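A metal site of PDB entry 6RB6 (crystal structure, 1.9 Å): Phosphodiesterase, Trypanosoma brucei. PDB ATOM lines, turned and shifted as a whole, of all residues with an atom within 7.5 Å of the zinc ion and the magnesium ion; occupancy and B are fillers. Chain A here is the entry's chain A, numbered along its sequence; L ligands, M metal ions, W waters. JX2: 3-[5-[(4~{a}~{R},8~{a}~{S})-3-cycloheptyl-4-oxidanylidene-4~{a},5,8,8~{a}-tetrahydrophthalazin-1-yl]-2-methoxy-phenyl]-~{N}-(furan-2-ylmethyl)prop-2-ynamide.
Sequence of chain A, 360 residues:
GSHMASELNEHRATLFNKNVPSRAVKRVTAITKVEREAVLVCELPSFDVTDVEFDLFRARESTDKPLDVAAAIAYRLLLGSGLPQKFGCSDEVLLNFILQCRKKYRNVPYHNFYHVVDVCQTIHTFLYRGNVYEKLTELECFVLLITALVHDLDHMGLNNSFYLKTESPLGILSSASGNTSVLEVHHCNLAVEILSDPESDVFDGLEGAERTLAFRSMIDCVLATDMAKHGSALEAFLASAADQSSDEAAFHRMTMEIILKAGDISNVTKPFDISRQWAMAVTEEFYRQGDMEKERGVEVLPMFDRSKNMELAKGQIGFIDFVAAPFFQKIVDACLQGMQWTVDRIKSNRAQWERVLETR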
ATOM      1  N   TYR A 110      -4.335  17.348   3.922  1.00  0.00           N
ATOM      2  CA  TYR A 110      -5.539  17.280   3.047  1.00  0.00           C
ATOM      3  C   TYR A 110      -5.732  18.566   2.217  1.00  0.00           C
ATOM      4  O   TYR A 110      -5.889  18.450   0.979  1.00  0.00           O
ATOM      5  CB  TYR A 110      -6.756  16.923   3.904  1.00  0.00           C
ATOM      6  CG  TYR A 110      -8.030  16.835   3.108  1.00  0.00           C
ATOM      7  CD1 TYR A 110      -8.822  17.950   2.919  1.00  0.00           C
ATOM      8  CD2 TYR A 110      -8.449  15.627   2.554  1.00  0.00           C
ATOM      9  CE1 TYR A 110      -9.988  17.891   2.143  1.00  0.00           C
ATOM     10  CE2 TYR A 110      -9.613  15.553   1.795  1.00  0.00           C
ATOM     11  CZ  TYR A 110     -10.390  16.685   1.584  1.00  0.00           C
ATOM     12  OH  TYR A 110     -11.535  16.616   0.865  1.00  0.00           O
ATOM     13  N   HIS A 111      -5.782  19.748   2.845  1.00  0.00           N
ATOM     14  CA  HIS A 111      -6.125  21.048   2.190  1.00  0.00           C
ATOM     15  C   HIS A 111      -4.896  21.636   1.480  1.00  0.00           C
ATOM     16  O   HIS A 111      -4.515  22.783   1.797  1.00  0.00           O
ATOM     17  CB  HIS A 111      -6.751  21.980   3.236  1.00  0.00           C
ATOM     18  CG  HIS A 111      -8.108  21.572   3.706  1.00  0.00           C
ATOM     19  ND1 HIS A 111      -8.320  20.945   4.922  1.00  0.00           N
ATOM     20  CD2 HIS A 111      -9.327  21.698   3.137  1.00  0.00           C
ATOM     21  CE1 HIS A 111      -9.613  20.717   5.088  1.00  0.00           C
ATOM     22  NE2 HIS A 111     -10.248  21.138   3.999  1.00  0.00           N
ATOM     23  N   HIS A 115      -5.777  18.517  -3.326  1.00  0.00           N
ATOM     24  CA  HIS A 115      -7.232  18.689  -3.085  1.00  0.00           C
ATOM     25  C   HIS A 115      -7.870  19.607  -4.155  1.00  0.00           C
ATOM     26  O   HIS A 115      -8.943  19.271  -4.670  1.00  0.00           O
ATOM     27  CB  HIS A 115      -7.491  19.187  -1.658  1.00  0.00           C
ATOM     28  CG  HIS A 115      -8.869  19.695  -1.436  1.00  0.00           C
ATOM     29  ND1 HIS A 115     -10.010  18.875  -1.511  1.00  0.00           N
ATOM     30  CD2 HIS A 115      -9.320  20.930  -1.094  1.00  0.00           C
ATOM     31  CE1 HIS A 115     -11.076  19.609  -1.200  1.00  0.00           C
ATOM     32  NE2 HIS A 115     -10.677  20.887  -0.982  1.00  0.00           N
ATOM     33  N   VAL A 116      -7.275  20.747  -4.464  1.00  0.00           N
ATOM     34  CA  VAL A 116      -7.912  21.737  -5.383  1.00  0.00           C
ATOM     35  C   VAL A 116      -7.818  21.254  -6.820  1.00  0.00           C
ATOM     36  O   VAL A 116      -8.807  21.422  -7.559  1.00  0.00           O
ATOM     37  CB  VAL A 116      -7.344  23.142  -5.148  1.00  0.00           C
ATOM     38  CG1 VAL A 116      -7.465  23.514  -3.686  1.00  0.00           C
ATOM     39  CG2 VAL A 116      -5.905  23.324  -5.637  1.00  0.00           C
ATOM     40  N   VAL A 119     -10.676  18.793  -6.976  1.00  0.00           N
ATOM     41  CA  VAL A 119     -12.006  19.482  -7.068  1.00  0.00           C
ATOM     42  C   VAL A 119     -12.223  20.025  -8.488  1.00  0.00           C
ATOM     43  O   VAL A 119     -13.346  19.884  -9.010  1.00  0.00           O
ATOM     44  CB  VAL A 119     -12.111  20.594  -6.001  1.00  0.00           C
ATOM     45  CG1 VAL A 119     -13.330  21.480  -6.204  1.00  0.00           C
ATOM     46  CG2 VAL A 119     -12.124  19.977  -4.616  1.00  0.00           C
ATOM     47  N   ALA A 148     -12.215  26.471  -8.645  1.00  0.00           N
ATOM     48  CA  ALA A 148     -11.764  25.234  -7.955  1.00  0.00           C
ATOM     49  C   ALA A 148     -10.313  25.429  -7.481  1.00  0.00           C
ATOM     50  O   ALA A 148      -9.992  25.032  -6.333  1.00  0.00           O
ATOM     51  CB  ALA A 148     -11.913  24.068  -8.888  1.00  0.00           C
ATOM     52  N   HIS A 151     -10.057  28.056  -4.414  1.00  0.00           N
ATOM     53  CA  HIS A 151     -11.013  27.784  -3.290  1.00  0.00           C
ATOM     54  C   HIS A 151     -10.408  27.640  -1.877  1.00  0.00           C
ATOM     55  O   HIS A 151     -11.142  27.942  -0.913  1.00  0.00           O
ATOM     56  CB  HIS A 151     -11.905  26.580  -3.629  1.00  0.00           C
ATOM     57  CG  HIS A 151     -11.471  25.310  -2.983  1.00  0.00           C
ATOM     58  ND1 HIS A 151     -10.805  24.316  -3.670  1.00  0.00           N
ATOM     59  CD2 HIS A 151     -11.602  24.871  -1.717  1.00  0.00           C
ATOM     60  CE1 HIS A 151     -10.547  23.308  -2.857  1.00  0.00           C
ATOM     61  NE2 HIS A 151     -11.022  23.627  -1.654  1.00  0.00           N
ATOM     62  N   ASP A 152      -9.161  27.190  -1.747  1.00  0.00           N
ATOM     63  CA  ASP A 152      -8.551  26.896  -0.422  1.00  0.00           C
ATOM     64  C   ASP A 152      -7.105  27.418  -0.366  1.00  0.00           C
ATOM     65  O   ASP A 152      -6.263  26.741   0.254  1.00  0.00           O
ATOM     66  CB  ASP A 152      -8.615  25.403  -0.102  1.00  0.00           C
ATOM     67  CG  ASP A 152      -9.963  24.974   0.459  1.00  0.00           C
ATOM     68  OD1 ASP A 152     -10.631  25.817   1.086  1.00  0.00           O
ATOM     69  OD2 ASP A 152     -10.330  23.796   0.278  1.00  0.00           O
ATOM     70  N   LEU A 153      -6.844  28.570  -0.999  1.00  0.00           N
ATOM     71  CA  LEU A 153      -5.490  29.201  -0.992  1.00  0.00           C
ATOM     72  C   LEU A 153      -4.974  29.469   0.427  1.00  0.00           C
ATOM     73  O   LEU A 153      -5.687  30.055   1.178  1.00  0.00           O
ATOM     74  CB  LEU A 153      -5.504  30.515  -1.797  1.00  0.00           C
ATOM     75  CG  LEU A 153      -5.659  30.394  -3.313  1.00  0.00           C
ATOM     76  CD1 LEU A 153      -5.920  31.748  -3.929  1.00  0.00           C
ATOM     77  CD2 LEU A 153      -4.446  29.750  -3.953  1.00  0.00           C
ATOM     78  N   HIS A 155      -4.500  27.485   2.988  1.00  0.00           N
ATOM     79  CA  HIS A 155      -5.120  26.743   4.125  1.00  0.00           C
ATOM     80  C   HIS A 155      -4.016  26.220   5.060  1.00  0.00           C
ATOM     81  O   HIS A 155      -3.006  25.781   4.559  1.00  0.00           O
ATOM     82  CB  HIS A 155      -6.012  25.604   3.612  1.00  0.00           C
ATOM     83  CG  HIS A 155      -7.075  25.166   4.565  1.00  0.00           C
ATOM     84  ND1 HIS A 155      -6.796  24.591   5.763  1.00  0.00           N
ATOM     85  CD2 HIS A 155      -8.418  25.204   4.482  1.00  0.00           C
ATOM     86  CE1 HIS A 155      -7.908  24.312   6.382  1.00  0.00           C
ATOM     87  NE2 HIS A 155      -8.917  24.673   5.613  1.00  0.00           N
ATOM     88  N   LEU A 183     -11.622  31.597   7.015  1.00  0.00           N
ATOM     89  CA  LEU A 183     -10.790  31.027   5.942  1.00  0.00           C
ATOM     90  C   LEU A 183     -11.305  31.496   4.579  1.00  0.00           C
ATOM     91  O   LEU A 183     -10.484  31.838   3.745  1.00  0.00           O
ATOM     92  CB  LEU A 183     -10.818  29.513   6.040  1.00  0.00           C
ATOM     93  CG  LEU A 183      -9.937  28.948   7.151  1.00  0.00           C
ATOM     94  CD1 LEU A 183     -10.186  27.474   7.316  1.00  0.00           C
ATOM     95  CD2 LEU A 183      -8.472  29.236   6.879  1.00  0.00           C
ATOM     96  N   GLU A 184     -12.634  31.489   4.376  1.00  0.00           N
ATOM     97  CA  GLU A 184     -13.201  31.662   2.994  1.00  0.00           C
ATOM     98  C   GLU A 184     -12.938  33.106   2.537  1.00  0.00           C
ATOM     99  O   GLU A 184     -12.499  33.292   1.382  1.00  0.00           O
ATOM    100  CB  GLU A 184     -14.664  31.203   2.944  1.00  0.00           C
ATOM    101  CG  GLU A 184     -14.866  29.695   3.129  1.00  0.00           C
ATOM    102  CD  GLU A 184     -14.770  29.177   4.563  1.00  0.00           C
ATOM    103  OE1 GLU A 184     -14.899  30.009   5.537  1.00  0.00           O
ATOM    104  OE2 GLU A 184     -14.511  27.940   4.713  1.00  0.00           O
ATOM    105  N   HIS A 187      -9.197  33.151   1.515  1.00  0.00           N
ATOM    106  CA  HIS A 187      -8.978  32.492   0.184  1.00  0.00           C
ATOM    107  C   HIS A 187      -9.346  33.509  -0.941  1.00  0.00           C
ATOM    108  O   HIS A 187      -8.590  33.626  -1.951  1.00  0.00           O
ATOM    109  CB  HIS A 187      -9.789  31.178   0.062  1.00  0.00           C
ATOM    110  CG  HIS A 187      -9.613  30.153   1.163  1.00  0.00           C
ATOM    111  ND1 HIS A 187      -8.385  29.841   1.745  1.00  0.00           N
ATOM    112  CD2 HIS A 187     -10.517  29.334   1.737  1.00  0.00           C
ATOM    113  CE1 HIS A 187      -8.590  28.917   2.687  1.00  0.00           C
ATOM    114  NE2 HIS A 187      -9.885  28.582   2.687  1.00  0.00           N
ATOM    115  N   VAL A 222     -16.755  30.679  -3.572  1.00  0.00           N
ATOM    116  CA  VAL A 222     -15.789  30.415  -2.471  1.00  0.00           C
ATOM    117  C   VAL A 222     -16.474  30.638  -1.108  1.00  0.00           C
ATOM    118  O   VAL A 222     -16.302  29.803  -0.147  1.00  0.00           O
ATOM    119  CB  VAL A 222     -14.496  31.247  -2.626  1.00  0.00           C
ATOM    120  CG1 VAL A 222     -13.555  31.024  -1.458  1.00  0.00           C
ATOM    121  CG2 VAL A 222     -13.776  30.942  -3.915  1.00  0.00           C
ATOM    122  N   THR A 225     -18.580  27.784   0.297  1.00  0.00           N
ATOM    123  CA  THR A 225     -17.920  26.529   0.747  1.00  0.00           C
ATOM    124  C   THR A 225     -17.838  26.443   2.269  1.00  0.00           C
ATOM    125  O   THR A 225     -17.481  25.372   2.758  1.00  0.00           O
ATOM    126  CB  THR A 225     -16.539  26.297   0.131  1.00  0.00           C
ATOM    127  OG1 THR A 225     -15.634  27.359   0.475  1.00  0.00           O
ATOM    128  CG2 THR A 225     -16.644  26.080  -1.383  1.00  0.00           C
ATOM    129  N   ASP A 226     -18.159  27.482   3.041  1.00  0.00           N
ATOM    130  CA  ASP A 226     -18.163  27.399   4.529  1.00  0.00           C
ATOM    131  C   ASP A 226     -19.288  26.452   4.953  1.00  0.00           C
ATOM    132  O   ASP A 226     -20.452  26.758   4.677  1.00  0.00           O
ATOM    133  CB  ASP A 226     -18.313  28.787   5.150  1.00  0.00           C
ATOM    134  CG  ASP A 226     -18.398  28.828   6.677  1.00  0.00           C
ATOM    135  OD1 ASP A 226     -18.540  27.780   7.296  1.00  0.00           O
ATOM    136  OD2 ASP A 226     -18.312  29.957   7.236  1.00  0.00           O
ATOM    137  N   MET A 227     -18.974  25.329   5.588  1.00  0.00           N
ATOM    138  CA  MET A 227     -20.017  24.301   5.884  1.00  0.00           C
ATOM    139  C   MET A 227     -21.077  24.805   6.900  1.00  0.00           C
ATOM    140  O   MET A 227     -22.180  24.204   6.971  1.00  0.00           O
ATOM    141  CB  MET A 227     -19.384  22.975   6.305  1.00  0.00           C
ATOM    142  CG  MET A 227     -18.744  22.217   5.145  1.00  0.00           C
ATOM    143  SD  MET A 227     -19.984  21.651   3.893  1.00  0.00           S
ATOM    144  CE  MET A 227     -20.898  20.488   4.907  1.00  0.00           C
ATOM    145  N   LEU A 260     -19.712  23.850  -6.844  1.00  0.00           N
ATOM    146  CA  LEU A 260     -18.409  23.977  -6.143  1.00  0.00           C
ATOM    147  C   LEU A 260     -18.520  23.173  -4.838  1.00  0.00           C
ATOM    148  O   LEU A 260     -17.560  22.425  -4.519  1.00  0.00           O
ATOM    149  CB  LEU A 260     -17.963  25.420  -5.894  1.00  0.00           C
ATOM    150  CG  LEU A 260     -16.625  25.568  -5.157  1.00  0.00           C
ATOM    151  CD1 LEU A 260     -15.489  24.922  -5.948  1.00  0.00           C
ATOM    152  CD2 LEU A 260     -16.258  27.023  -4.884  1.00  0.00           C
ATOM    153  N   GLY A 263     -18.295  19.435  -5.559  1.00  0.00           N
ATOM    154  CA  GLY A 263     -16.869  19.083  -5.804  1.00  0.00           C
ATOM    155  C   GLY A 263     -16.101  18.998  -4.501  1.00  0.00           C
ATOM    156  O   GLY A 263     -15.265  18.093  -4.311  1.00  0.00           O
ATOM    157  N   ASP A 264     -16.333  19.935  -3.611  1.00  0.00           N
ATOM    158  CA  ASP A 264     -15.626  20.037  -2.316  1.00  0.00           C
ATOM    159  C   ASP A 264     -15.928  18.822  -1.399  1.00  0.00           C
ATOM    160  O   ASP A 264     -15.007  18.442  -0.661  1.00  0.00           O
ATOM    161  CB  ASP A 264     -15.994  21.333  -1.593  1.00  0.00           C
ATOM    162  CG  ASP A 264     -14.931  21.846  -0.657  1.00  0.00           C
ATOM    163  OD1 ASP A 264     -13.739  21.544  -0.903  1.00  0.00           O
ATOM    164  OD2 ASP A 264     -15.289  22.626   0.278  1.00  0.00           O
ATOM    165  N   ILE A 265     -17.129  18.220  -1.433  1.00  0.00           N
ATOM    166  CA  ILE A 265     -17.452  17.018  -0.607  1.00  0.00           C
ATOM    167  C   ILE A 265     -17.578  15.765  -1.501  1.00  0.00           C
ATOM    168  O   ILE A 265     -18.300  14.846  -1.074  1.00  0.00           O
ATOM    169  CB  ILE A 265     -18.688  17.254   0.288  1.00  0.00           C
ATOM    170  CG1 ILE A 265     -19.954  17.502  -0.514  1.00  0.00           C
ATOM    171  CG2 ILE A 265     -18.452  18.403   1.271  1.00  0.00           C
ATOM    172  CD1 ILE A 265     -21.189  17.443   0.339  1.00  0.00           C
HETATM  173  C1  JX2 L   1     -13.525  12.340   3.540  1.00  0.00           C
HETATM  174  N2  JX2 L   1     -15.943  18.234   7.144  1.00  0.00           N
HETATM  175  C3  JX2 L   1     -14.521  14.984   3.920  1.00  0.00           C
HETATM  176  C5  JX2 L   1     -15.099  16.676   5.558  1.00  0.00           C
HETATM  177  C6  JX2 L   1     -15.239  15.669   6.533  1.00  0.00           C
HETATM  178  C7  JX2 L   1     -15.017  14.327   6.205  1.00  0.00           C
HETATM  179  C9  JX2 L   1     -15.155  12.508   8.120  1.00  0.00           C
HETATM  180  C10 JX2 L   1     -15.060  11.518   9.143  1.00  0.00           C
HETATM  181  C11 JX2 L   1     -16.164  13.201  10.589  1.00  0.00           C
HETATM  182  C12 JX2 L   1     -17.631  13.394  10.484  1.00  0.00           C
HETATM  183  C13 JX2 L   1     -18.358  14.479  10.118  1.00  0.00           C
HETATM  184  C14 JX2 L   1     -19.746  14.118  10.250  1.00  0.00           C
HETATM  185  C15 JX2 L   1     -19.768  12.836  10.726  1.00  0.00           C
HETATM  186  C16 JX2 L   1     -15.389  18.081   5.995  1.00  0.00           C
HETATM  187  C17 JX2 L   1     -17.526  19.539   8.430  1.00  0.00           C
HETATM  188  C18 JX2 L   1     -17.023  19.206   9.857  1.00  0.00           C
HETATM  189  C19 JX2 L   1     -17.706  18.045  10.581  1.00  0.00           C
HETATM  190  C2  JX2 L   1     -14.653  13.979   4.884  1.00  0.00           C
HETATM  191  C20 JX2 L   1     -19.206  18.121  10.819  1.00  0.00           C
HETATM  192  C21 JX2 L   1     -19.959  19.247  10.109  1.00  0.00           C
HETATM  193  C22 JX2 L   1     -20.071  19.064   8.622  1.00  0.00           C
HETATM  194  C23 JX2 L   1     -18.732  18.711   7.949  1.00  0.00           C
HETATM  195  C24 JX2 L   1     -15.836  20.682   6.951  1.00  0.00           C
HETATM  196  C25 JX2 L   1     -14.707  20.508   5.963  1.00  0.00           C
HETATM  197  C26 JX2 L   1     -14.403  21.785   5.161  1.00  0.00           C
HETATM  198  C27 JX2 L   1     -15.160  21.877   3.877  1.00  0.00           C
HETATM  199  C28 JX2 L   1     -15.911  20.905   3.383  1.00  0.00           C
HETATM  200  C29 JX2 L   1     -16.112  19.578   4.042  1.00  0.00           C
HETATM  201  C30 JX2 L   1     -15.022  19.265   5.093  1.00  0.00           C
HETATM  202  C4  JX2 L   1     -14.738  16.319   4.259  1.00  0.00           C
HETATM  203  C8  JX2 L   1     -15.138  13.325   7.239  1.00  0.00           C
HETATM  204  N1  JX2 L   1     -15.647  11.852  10.313  1.00  0.00           N
HETATM  205  N3  JX2 L   1     -16.395  19.486   7.452  1.00  0.00           N
HETATM  206  O1  JX2 L   1     -14.421  12.654   4.627  1.00  0.00           O
HETATM  207  O2  JX2 L   1     -14.493  10.440   8.924  1.00  0.00           O
HETATM  208  O3  JX2 L   1     -18.476  12.382  10.879  1.00  0.00           O
HETATM  209  O4  JX2 L   1     -16.214  21.784   7.334  1.00  0.00           O
HETATM  210 ZN    ZN M   1     -11.930  22.545  -0.239  1.00  0.00          ZN
HETATM  211 MG    MG M   2     -12.455  25.440   2.208  1.00  0.00          MG
HETATM  212  O   HOH W   1     -11.719  26.655   3.608  1.00  0.00           O
HETATM  213  O   HOH W   2     -12.996  23.866   0.893  1.00  0.00           O
HETATM  214  O   HOH W   3     -14.210  25.672   3.038  1.00  0.00           O
HETATM  215  O   HOH W   4     -12.221  21.396   1.762  1.00  0.00           O
HETATM  216  O   HOH W   5     -12.062  23.791   3.511  1.00  0.00           O
HETATM  217  O   HOH W   6     -12.947  27.038   1.166  1.00  0.00           O
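Of the 21 residues printed, 4 come within 4 Å of the zinc ion.
The magnesium ion is bound by water W3, water W6, water W1, water W2, water W5 and the side-chain carboxylate of Asp 152.
The magnesium ion has six donor atoms within binding distance.
The zinc ion is bound by a ring nitrogen (NE2) of His 151 (2.0 Å), water W2 (2.0 Å), the side-chain carboxylate (OD2) of Asp 152 (2.1 Å), the side-chain carboxylate (OD1) of Asp 264 (2.2 Å), a ring nitrogen (NE2) of His 115 (2.2 Å) and water W4 (2.3 Å).
The zinc ion has six donor atoms within binding distance.
OD1 of Asp 152 sits close to NE2 of His 187 (3.3 Å).
O of Ala 148 sits at hydrogen-bond distance from ND1 of His 151 (2.9 Å).
Water W3 bridges OE2 of Glu 184 and O of Thr 225.
Water W6 lies within hydrogen-bond range of OG1 of Thr 225 and O of His 151.
Water W1 lies within hydrogen-bond range of NE2 of His 187 (2.8 Å) and OE2 of Glu 184 (3.3 Å).
The nearest printed residue that does not touch the magnesium ion is His 151 (4.1 Å).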
